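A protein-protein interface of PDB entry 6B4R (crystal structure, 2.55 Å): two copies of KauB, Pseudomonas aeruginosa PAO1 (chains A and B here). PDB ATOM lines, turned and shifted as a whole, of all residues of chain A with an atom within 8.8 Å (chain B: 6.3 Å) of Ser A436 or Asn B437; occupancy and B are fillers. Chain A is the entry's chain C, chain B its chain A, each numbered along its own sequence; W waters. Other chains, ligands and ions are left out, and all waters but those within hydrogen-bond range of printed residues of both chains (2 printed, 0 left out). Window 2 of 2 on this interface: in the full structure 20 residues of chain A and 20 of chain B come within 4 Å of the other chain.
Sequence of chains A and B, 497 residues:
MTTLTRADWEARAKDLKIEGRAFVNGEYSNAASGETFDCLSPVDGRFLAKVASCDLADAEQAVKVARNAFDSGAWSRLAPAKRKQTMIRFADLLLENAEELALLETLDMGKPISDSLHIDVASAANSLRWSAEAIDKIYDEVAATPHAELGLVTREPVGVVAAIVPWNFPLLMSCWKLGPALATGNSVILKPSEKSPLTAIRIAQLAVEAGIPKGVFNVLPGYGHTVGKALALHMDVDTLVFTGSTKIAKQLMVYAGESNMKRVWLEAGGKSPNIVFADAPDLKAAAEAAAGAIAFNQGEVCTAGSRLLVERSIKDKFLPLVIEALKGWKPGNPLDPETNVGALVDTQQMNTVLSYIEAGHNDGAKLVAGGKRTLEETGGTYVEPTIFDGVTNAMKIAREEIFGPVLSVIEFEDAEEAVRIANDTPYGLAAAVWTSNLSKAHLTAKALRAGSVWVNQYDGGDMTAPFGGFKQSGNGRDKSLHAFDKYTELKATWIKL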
ATOM      1  N   PHE A 277       2.318  -3.703 -18.024  1.00  0.00           N
ATOM      2  CA  PHE A 277       1.186  -3.173 -18.775  1.00  0.00           C
ATOM      3  C   PHE A 277       1.647  -2.298 -19.932  1.00  0.00           C
ATOM      4  O   PHE A 277       2.829  -1.968 -20.047  1.00  0.00           O
ATOM      5  CB  PHE A 277       0.251  -2.378 -17.862  1.00  0.00           C
ATOM      6  CG  PHE A 277      -0.638  -3.236 -17.007  1.00  0.00           C
ATOM      7  CD1 PHE A 277      -1.882  -3.640 -17.466  1.00  0.00           C
ATOM      8  CD2 PHE A 277      -0.235  -3.631 -15.742  1.00  0.00           C
ATOM      9  CE1 PHE A 277      -2.706  -4.427 -16.680  1.00  0.00           C
ATOM     10  CE2 PHE A 277      -1.054  -4.417 -14.952  1.00  0.00           C
ATOM     11  CZ  PHE A 277      -2.291  -4.816 -15.421  1.00  0.00           C
ATOM     12  N   ALA A 278       0.700  -1.922 -20.784  1.00  0.00           N
ATOM     13  CA  ALA A 278       0.990  -1.095 -21.949  1.00  0.00           C
ATOM     14  C   ALA A 278       1.387   0.321 -21.552  1.00  0.00           C
ATOM     15  O   ALA A 278       2.273   0.917 -22.163  1.00  0.00           O
ATOM     16  CB  ALA A 278      -0.207  -1.063 -22.883  1.00  0.00           C
ATOM     17  N   ASP A 279       0.731   0.850 -20.523  1.00  0.00           N
ATOM     18  CA  ASP A 279       0.958   2.229 -20.100  1.00  0.00           C
ATOM     19  C   ASP A 279       2.064   2.362 -19.058  1.00  0.00           C
ATOM     20  O   ASP A 279       2.031   3.266 -18.224  1.00  0.00           O
ATOM     21  CB  ASP A 279      -0.338   2.869 -19.588  1.00  0.00           C
ATOM     22  CG  ASP A 279      -1.013   2.052 -18.496  1.00  0.00           C
ATOM     23  OD1 ASP A 279      -0.328   1.253 -17.821  1.00  0.00           O
ATOM     24  OD2 ASP A 279      -2.238   2.215 -18.308  1.00  0.00           O
ATOM     25  N   ALA A 280       3.035   1.459 -19.105  1.00  0.00           N
ATOM     26  CA  ALA A 280       4.196   1.557 -18.230  1.00  0.00           C
ATOM     27  C   ALA A 280       4.937   2.858 -18.520  1.00  0.00           C
ATOM     28  O   ALA A 280       5.025   3.275 -19.674  1.00  0.00           O
ATOM     29  CB  ALA A 280       5.114   0.357 -18.424  1.00  0.00           C
ATOM     30  N   PRO A 281       5.461   3.509 -17.468  1.00  0.00           N
ATOM     31  CA  PRO A 281       6.171   4.789 -17.590  1.00  0.00           C
ATOM     32  C   PRO A 281       7.341   4.718 -18.569  1.00  0.00           C
ATOM     33  O   PRO A 281       7.581   5.670 -19.309  1.00  0.00           O
ATOM     34  CB  PRO A 281       6.695   5.031 -16.170  1.00  0.00           C
ATOM     35  CG  PRO A 281       5.770   4.273 -15.288  1.00  0.00           C
ATOM     36  CD  PRO A 281       5.388   3.050 -16.070  1.00  0.00           C
ATOM     37  N   ASP A 282       8.054   3.595 -18.566  1.00  0.00           N
ATOM     38  CA  ASP A 282       9.215   3.415 -19.431  1.00  0.00           C
ATOM     39  C   ASP A 282       9.407   1.939 -19.773  1.00  0.00           C
ATOM     40  O   ASP A 282       9.845   1.150 -18.936  1.00  0.00           O
ATOM     41  CB  ASP A 282      10.468   3.976 -18.752  1.00  0.00           C
ATOM     42  CG  ASP A 282      11.689   3.945 -19.652  1.00  0.00           C
ATOM     43  OD1 ASP A 282      11.535   3.692 -20.866  1.00  0.00           O
ATOM     44  OD2 ASP A 282      12.805   4.190 -19.146  1.00  0.00           O
ATOM     45  N   VAL A 433       4.327  -4.844 -10.632  1.00  0.00           N
ATOM     46  CA  VAL A 433       3.393  -4.184 -11.537  1.00  0.00           C
ATOM     47  C   VAL A 433       4.038  -2.970 -12.196  1.00  0.00           C
ATOM     48  O   VAL A 433       4.622  -2.126 -11.520  1.00  0.00           O
ATOM     49  CB  VAL A 433       2.124  -3.723 -10.804  1.00  0.00           C
ATOM     50  CG1 VAL A 433       1.106  -3.202 -11.802  1.00  0.00           C
ATOM     51  CG2 VAL A 433       1.536  -4.862  -9.981  1.00  0.00           C
ATOM     52  N   TRP A 434       3.923  -2.888 -13.519  1.00  0.00           N
ATOM     53  CA  TRP A 434       4.484  -1.772 -14.275  1.00  0.00           C
ATOM     54  C   TRP A 434       3.396  -0.989 -14.998  1.00  0.00           C
ATOM     55  O   TRP A 434       2.861  -1.444 -16.010  1.00  0.00           O
ATOM     56  CB  TRP A 434       5.516  -2.273 -15.285  1.00  0.00           C
ATOM     57  CG  TRP A 434       6.727  -2.873 -14.648  1.00  0.00           C
ATOM     58  CD1 TRP A 434       6.855  -4.142 -14.159  1.00  0.00           C
ATOM     59  CD2 TRP A 434       7.985  -2.227 -14.424  1.00  0.00           C
ATOM     60  NE1 TRP A 434       8.116  -4.325 -13.645  1.00  0.00           N
ATOM     61  CE2 TRP A 434       8.830  -3.166 -13.797  1.00  0.00           C
ATOM     62  CE3 TRP A 434       8.480  -0.947 -14.693  1.00  0.00           C
ATOM     63  CZ2 TRP A 434      10.139  -2.863 -13.436  1.00  0.00           C
ATOM     64  CZ3 TRP A 434       9.782  -0.651 -14.335  1.00  0.00           C
ATOM     65  CH2 TRP A 434      10.596  -1.604 -13.713  1.00  0.00           C
ATOM     66  N   THR A 435       3.079   0.191 -14.474  1.00  0.00           N
ATOM     67  CA  THR A 435       2.040   1.037 -15.052  1.00  0.00           C
ATOM     68  C   THR A 435       2.178   2.472 -14.558  1.00  0.00           C
ATOM     69  O   THR A 435       2.836   2.730 -13.554  1.00  0.00           O
ATOM     70  CB  THR A 435       0.631   0.517 -14.701  1.00  0.00           C
ATOM     71  OG1 THR A 435      -0.362   1.416 -15.213  1.00  0.00           O
ATOM     72  CG2 THR A 435       0.471   0.395 -13.199  1.00  0.00           C
ATOM     73  N   SER A 436       1.556   3.406 -15.269  1.00  0.00           N
ATOM     74  CA  SER A 436       1.589   4.804 -14.862  1.00  0.00           C
ATOM     75  C   SER A 436       0.227   5.261 -14.350  1.00  0.00           C
ATOM     76  O   SER A 436       0.080   6.385 -13.869  1.00  0.00           O
ATOM     77  CB  SER A 436       2.035   5.685 -16.027  1.00  0.00           C
ATOM     78  OG  SER A 436       1.146   5.553 -17.118  1.00  0.00           O
ATOM     79  N   ASN A 437      -0.765   4.382 -14.458  1.00  0.00           N
ATOM     80  CA  ASN A 437      -2.119   4.688 -14.012  1.00  0.00           C
ATOM     81  C   ASN A 437      -2.277   4.495 -12.506  1.00  0.00           C
ATOM     82  O   ASN A 437      -1.966   3.430 -11.975  1.00  0.00           O
ATOM     83  CB  ASN A 437      -3.135   3.829 -14.768  1.00  0.00           C
ATOM     84  CG  ASN A 437      -4.570   4.184 -14.427  1.00  0.00           C
ATOM     85  OD1 ASN A 437      -5.200   3.541 -13.585  1.00  0.00           O
ATOM     86  ND2 ASN A 437      -5.095   5.216 -15.079  1.00  0.00           N
ATOM     87  N   LEU A 438      -2.757   5.534 -11.829  1.00  0.00           N
ATOM     88  CA  LEU A 438      -2.910   5.523 -10.375  1.00  0.00           C
ATOM     89  C   LEU A 438      -3.796   4.379  -9.879  1.00  0.00           C
ATOM     90  O   LEU A 438      -3.353   3.533  -9.098  1.00  0.00           O
ATOM     91  CB  LEU A 438      -3.473   6.866  -9.893  1.00  0.00           C
ATOM     92  CG  LEU A 438      -3.856   6.976  -8.415  1.00  0.00           C
ATOM     93  CD1 LEU A 438      -2.619   6.889  -7.533  1.00  0.00           C
ATOM     94  CD2 LEU A 438      -4.623   8.262  -8.144  1.00  0.00           C
ATOM     95  N   SER A 439      -5.045   4.358 -10.337  1.00  0.00           N
ATOM     96  CA  SER A 439      -6.011   3.358  -9.891  1.00  0.00           C
ATOM     97  C   SER A 439      -5.562   1.933 -10.200  1.00  0.00           C
ATOM     98  O   SER A 439      -5.655   1.051  -9.347  1.00  0.00           O
ATOM     99  CB  SER A 439      -7.386   3.614 -10.518  1.00  0.00           C
ATOM    100  OG  SER A 439      -7.965   4.810 -10.025  1.00  0.00           O
ATOM    101  N   LYS A 440      -5.076   1.714 -11.420  1.00  0.00           N
ATOM    102  CA  LYS A 440      -4.689   0.374 -11.855  1.00  0.00           C
ATOM    103  C   LYS A 440      -3.477  -0.147 -11.085  1.00  0.00           C
ATOM    104  O   LYS A 440      -3.400  -1.335 -10.774  1.00  0.00           O
ATOM    105  CB  LYS A 440      -4.440   0.331 -13.366  1.00  0.00           C
ATOM    106  CG  LYS A 440      -4.191  -1.069 -13.909  1.00  0.00           C
ATOM    107  CD  LYS A 440      -4.329  -1.119 -15.424  1.00  0.00           C
ATOM    108  CE  LYS A 440      -3.287  -0.258 -16.118  1.00  0.00           C
ATOM    109  NZ  LYS A 440      -3.479  -0.237 -17.597  1.00  0.00           N
ATOM    110  N   ALA A 441      -2.541   0.743 -10.770  1.00  0.00           N
ATOM    111  CA  ALA A 441      -1.372   0.369  -9.980  1.00  0.00           C
ATOM    112  C   ALA A 441      -1.762  -0.130  -8.589  1.00  0.00           C
ATOM    113  O   ALA A 441      -1.331  -1.204  -8.166  1.00  0.00           O
ATOM    114  CB  ALA A 441      -0.406   1.540  -9.868  1.00  0.00           C
ATOM    115  N   HIS A 442      -2.588   0.643  -7.889  1.00  0.00           N
ATOM    116  CA  HIS A 442      -2.970   0.310  -6.519  1.00  0.00           C
ATOM    117  C   HIS A 442      -3.941  -0.865  -6.428  1.00  0.00           C
ATOM    118  O   HIS A 442      -3.807  -1.718  -5.549  1.00  0.00           O
ATOM    119  CB  HIS A 442      -3.558   1.529  -5.803  1.00  0.00           C
ATOM    120  CG  HIS A 442      -2.534   2.548  -5.409  1.00  0.00           C
ATOM    121  ND1 HIS A 442      -1.643   2.348  -4.379  1.00  0.00           N
ATOM    122  CD2 HIS A 442      -2.265   3.780  -5.906  1.00  0.00           C
ATOM    123  CE1 HIS A 442      -0.865   3.409  -4.257  1.00  0.00           C
ATOM    124  NE2 HIS A 442      -1.223   4.293  -5.172  1.00  0.00           N
ATOM    125  N   VAL A 455       6.133  -1.820  -7.536  1.00  0.00           N
ATOM    126  CA  VAL A 455       5.471  -1.041  -8.576  1.00  0.00           C
ATOM    127  C   VAL A 455       6.460  -0.131  -9.293  1.00  0.00           C
ATOM    128  O   VAL A 455       7.125   0.694  -8.665  1.00  0.00           O
ATOM    129  CB  VAL A 455       4.323  -0.190  -8.003  1.00  0.00           C
ATOM    130  CG1 VAL A 455       3.642   0.599  -9.111  1.00  0.00           C
ATOM    131  CG2 VAL A 455       3.319  -1.076  -7.280  1.00  0.00           C
ATOM    132  N   ASN A 456       6.541  -0.291 -10.612  1.00  0.00           N
ATOM    133  CA  ASN A 456       7.468   0.465 -11.455  1.00  0.00           C
ATOM    134  C   ASN A 456       8.932   0.280 -11.053  1.00  0.00           C
ATOM    135  O   ASN A 456       9.754   1.181 -11.216  1.00  0.00           O
ATOM    136  CB  ASN A 456       7.080   1.947 -11.519  1.00  0.00           C
ATOM    137  CG  ASN A 456       5.718   2.161 -12.160  1.00  0.00           C
ATOM    138  OD1 ASN A 456       5.181   1.263 -12.811  1.00  0.00           O
ATOM    139  ND2 ASN A 456       5.156   3.353 -11.986  1.00  0.00           N
ATOM    140  N   ASP B 279      -5.145  15.425 -17.289  1.00  0.00           N
ATOM    141  CA  ASP B 279      -5.289  13.973 -17.330  1.00  0.00           C
ATOM    142  C   ASP B 279      -6.171  13.419 -16.212  1.00  0.00           C
ATOM    143  O   ASP B 279      -6.000  12.276 -15.791  1.00  0.00           O
ATOM    144  CB  ASP B 279      -3.915  13.284 -17.317  1.00  0.00           C
ATOM    145  CG  ASP B 279      -3.067  13.665 -16.106  1.00  0.00           C
ATOM    146  OD1 ASP B 279      -3.575  14.346 -15.190  1.00  0.00           O
ATOM    147  OD2 ASP B 279      -1.880  13.270 -16.069  1.00  0.00           O
ATOM    148  N   THR B 435      -5.975  13.759 -11.062  1.00  0.00           N
ATOM    149  CA  THR B 435      -5.093  13.227 -12.092  1.00  0.00           C
ATOM    150  C   THR B 435      -5.158  11.705 -12.080  1.00  0.00           C
ATOM    151  O   THR B 435      -5.488  11.099 -11.061  1.00  0.00           O
ATOM    152  CB  THR B 435      -3.632  13.685 -11.888  1.00  0.00           C
ATOM    153  OG1 THR B 435      -2.794  13.115 -12.903  1.00  0.00           O
ATOM    154  CG2 THR B 435      -3.120  13.257 -10.529  1.00  0.00           C
ATOM    155  N   SER B 436      -4.852  11.093 -13.219  1.00  0.00           N
ATOM    156  CA  SER B 436      -4.866   9.641 -13.331  1.00  0.00           C
ATOM    157  C   SER B 436      -3.450   9.084 -13.284  1.00  0.00           C
ATOM    158  O   SER B 436      -3.251   7.870 -13.228  1.00  0.00           O
ATOM    159  CB  SER B 436      -5.555   9.212 -14.626  1.00  0.00           C
ATOM    160  OG  SER B 436      -4.838   9.673 -15.757  1.00  0.00           O
ATOM    161  N   ASN B 437      -2.469   9.981 -13.303  1.00  0.00           N
ATOM    162  CA  ASN B 437      -1.067   9.590 -13.290  1.00  0.00           C
ATOM    163  C   ASN B 437      -0.578   9.225 -11.890  1.00  0.00           C
ATOM    164  O   ASN B 437      -0.750   9.994 -10.946  1.00  0.00           O
ATOM    165  CB  ASN B 437      -0.200  10.706 -13.879  1.00  0.00           C
ATOM    166  CG  ASN B 437       1.253  10.299 -14.020  1.00  0.00           C
ATOM    167  OD1 ASN B 437       2.073  10.550 -13.136  1.00  0.00           O
ATOM    168  ND2 ASN B 437       1.576   9.654 -15.134  1.00  0.00           N
ATOM    169  N   LEU B 438       0.036   8.052 -11.768  1.00  0.00           N
ATOM    170  CA  LEU B 438       0.510   7.551 -10.479  1.00  0.00           C
ATOM    171  C   LEU B 438       1.545   8.473  -9.835  1.00  0.00           C
ATOM    172  O   LEU B 438       1.375   8.912  -8.695  1.00  0.00           O
ATOM    173  CB  LEU B 438       1.088   6.142 -10.632  1.00  0.00           C
ATOM    174  CG  LEU B 438       1.686   5.518  -9.368  1.00  0.00           C
ATOM    175  CD1 LEU B 438       0.610   5.306  -8.318  1.00  0.00           C
ATOM    176  CD2 LEU B 438       2.396   4.213  -9.684  1.00  0.00           C
ATOM    177  N   SER B 439       2.613   8.766 -10.572  1.00  0.00           N
ATOM    178  CA  SER B 439       3.697   9.599 -10.061  1.00  0.00           C
ATOM    179  C   SER B 439       3.233  11.012  -9.720  1.00  0.00           C
ATOM    180  O   SER B 439       3.567  11.541  -8.659  1.00  0.00           O
ATOM    181  CB  SER B 439       4.848   9.670 -11.070  1.00  0.00           C
ATOM    182  OG  SER B 439       5.418   8.392 -11.294  1.00  0.00           O
ATOM    183  N   LYS B 440       2.466  11.620 -10.618  1.00  0.00           N
ATOM    184  CA  LYS B 440       2.057  13.008 -10.439  1.00  0.00           C
ATOM    185  C   LYS B 440       1.079  13.176  -9.279  1.00  0.00           C
ATOM    186  O   LYS B 440       1.101  14.194  -8.590  1.00  0.00           O
ATOM    187  CB  LYS B 440       1.471  13.584 -11.731  1.00  0.00           C
ATOM    188  CG  LYS B 440       1.249  15.088 -11.676  1.00  0.00           C
ATOM    189  CD  LYS B 440       1.016  15.671 -13.058  1.00  0.00           C
ATOM    190  CE  LYS B 440      -0.213  15.079 -13.714  1.00  0.00           C
ATOM    191  NZ  LYS B 440      -0.376  15.585 -15.101  1.00  0.00           N
ATOM    192  N   ALA B 441       0.231  12.176  -9.059  1.00  0.00           N
ATOM    193  CA  ALA B 441      -0.711  12.219  -7.943  1.00  0.00           C
ATOM    194  C   ALA B 441       0.008  12.222  -6.596  1.00  0.00           C
ATOM    195  O   ALA B 441      -0.301  13.030  -5.722  1.00  0.00           O
ATOM    196  CB  ALA B 441      -1.690  11.053  -8.021  1.00  0.00           C
ATOM    197  N   HIS B 442       0.974  11.322  -6.435  1.00  0.00           N
ATOM    198  CA  HIS B 442       1.687  11.188  -5.167  1.00  0.00           C
ATOM    199  C   HIS B 442       2.668  12.328  -4.901  1.00  0.00           C
ATOM    200  O   HIS B 442       2.686  12.898  -3.810  1.00  0.00           O
ATOM    201  CB  HIS B 442       2.396   9.833  -5.089  1.00  0.00           C
ATOM    202  CG  HIS B 442       1.470   8.686  -4.826  1.00  0.00           C
ATOM    203  ND1 HIS B 442       0.907   8.454  -3.590  1.00  0.00           N
ATOM    204  CD2 HIS B 442       0.996   7.716  -5.643  1.00  0.00           C
ATOM    205  CE1 HIS B 442       0.132   7.388  -3.653  1.00  0.00           C
ATOM    206  NE2 HIS B 442       0.166   6.921  -4.889  1.00  0.00           N
HETATM  207  O   HOH W   1       3.369   7.068 -12.928  1.00  0.00           O
HETATM  208  O   HOH W   2       5.913   5.754 -11.041  1.00  0.00           O
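Ser A436 touches Asn B437, and with the chains exchanged Asn A437 touches Ser B436.
Leu A438 touches His B442, and with the chains exchanged His A442 touches Leu B438.
Ala A441 touches Leu B438, but with the chains exchanged Leu A438 does not touch Ala B441 (4.1 Å).
His A442 touches its own counterpart, His B442.
9 positions are printed for both chains.
Water W2 bridges the side-chain amide nitrogen (ND2) of Asn A456 (2.7 Å) and the side-chain hydroxyl (OG) of Ser B439 (2.7 Å).
Water W1 bridges the side-chain hydroxyl (OG) of Ser B439 and the backbone carbonyl oxygen (O) of Ser A436.
Among the printed residues, pairs that only touch across the chains: Ser A436 with Ser B436, Ser A436 with Asn B437, Asn A437 with Ser B436, Leu A438 with Leu B438, Leu A438 with His B442, Ala A441 with Leu B438, His A442 with Leu B438, Val A455 with Leu B438 and Asn A456 with Leu B438.
A ring nitrogen (NE2) of His A442 is in hydrogen-bond range of a ring nitrogen (NE2) of His B442, at 3.0 Å.
The backbone carbonyl oxygen (O) of Ser B436 sits at hydrogen-bond distance from the backbone NH (N) of Leu A438.
The backbone NH (N) of Leu B438 lies within hydrogen-bond range of the backbone carbonyl oxygen (O) of Ser A436 (2.7 Å).
Ser A436 touches just these residues of chain B: Ser B436 (3.7 Å), Asn B437 (3.5 Å) and Leu B438 (2.7 Å).
Of chain A, only Ser A436 comes within 4 Å of Asn B437.
Of chain A, only Ser A436 (3.7 Å), Asn A437 (3.5 Å) and Leu A438 (2.8 Å) come within 4 Å of Ser B436.
Of the printed residues of chain B, Asn A437 touches Ser B436.
Of the printed residues of chain B, His A442 touches Leu B438 (3.8 Å) and His B442 (3.0 Å).
Printed residues of chain A within 4 Å of Leu B438: Ser A436, Leu A438, Ala A441, His A442, Val A455 and Asn A456.
Of the printed residues of chain B, Ala A441 touches Leu B438.
Of the printed residues of chain B, Val A455 touches Leu B438.
N of Asn B437 sits at hydrogen-bond distance from OG1 of Thr B435, at 3.2 Å.
The backbone carbonyl oxygen (O) of Thr A435 sits close to the side-chain amide oxygen (OD1) of Asn A456 (2.9 Å).
O of Asp A279 lies within hydrogen-bond range of OG of Ser A436 (2.7 Å).
The side-chain amide oxygen of Asn A437 is in hydrogen-bond range of the backbone NH of Lys A440, 2.8 Å away.
OD1 of Asn B437 is in hydrogen-bond range of N of Lys B440, at 2.8 Å.
The side-chain hydroxyl (OG1) of Thr A435 sits at hydrogen-bond distance from the backbone NH (N) of Asn A437, 3.1 Å away.
Of the 18 printed residues of chain A, 7 touch a printed residue of chain B.
Hydrophobic or aromatic side chains of chain A that line the printed part of chain B: Leu A438, Ala A441, His A442 and Val A455.
Hydrophobic or aromatic side chains of chain B that line the printed part of chain A: Leu B438 and His B442.
Along chain B the printed residues that touch a printed residue of chain A span positions 436 to 442.
Among the printed residues, 12 pairs touch across the chains.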
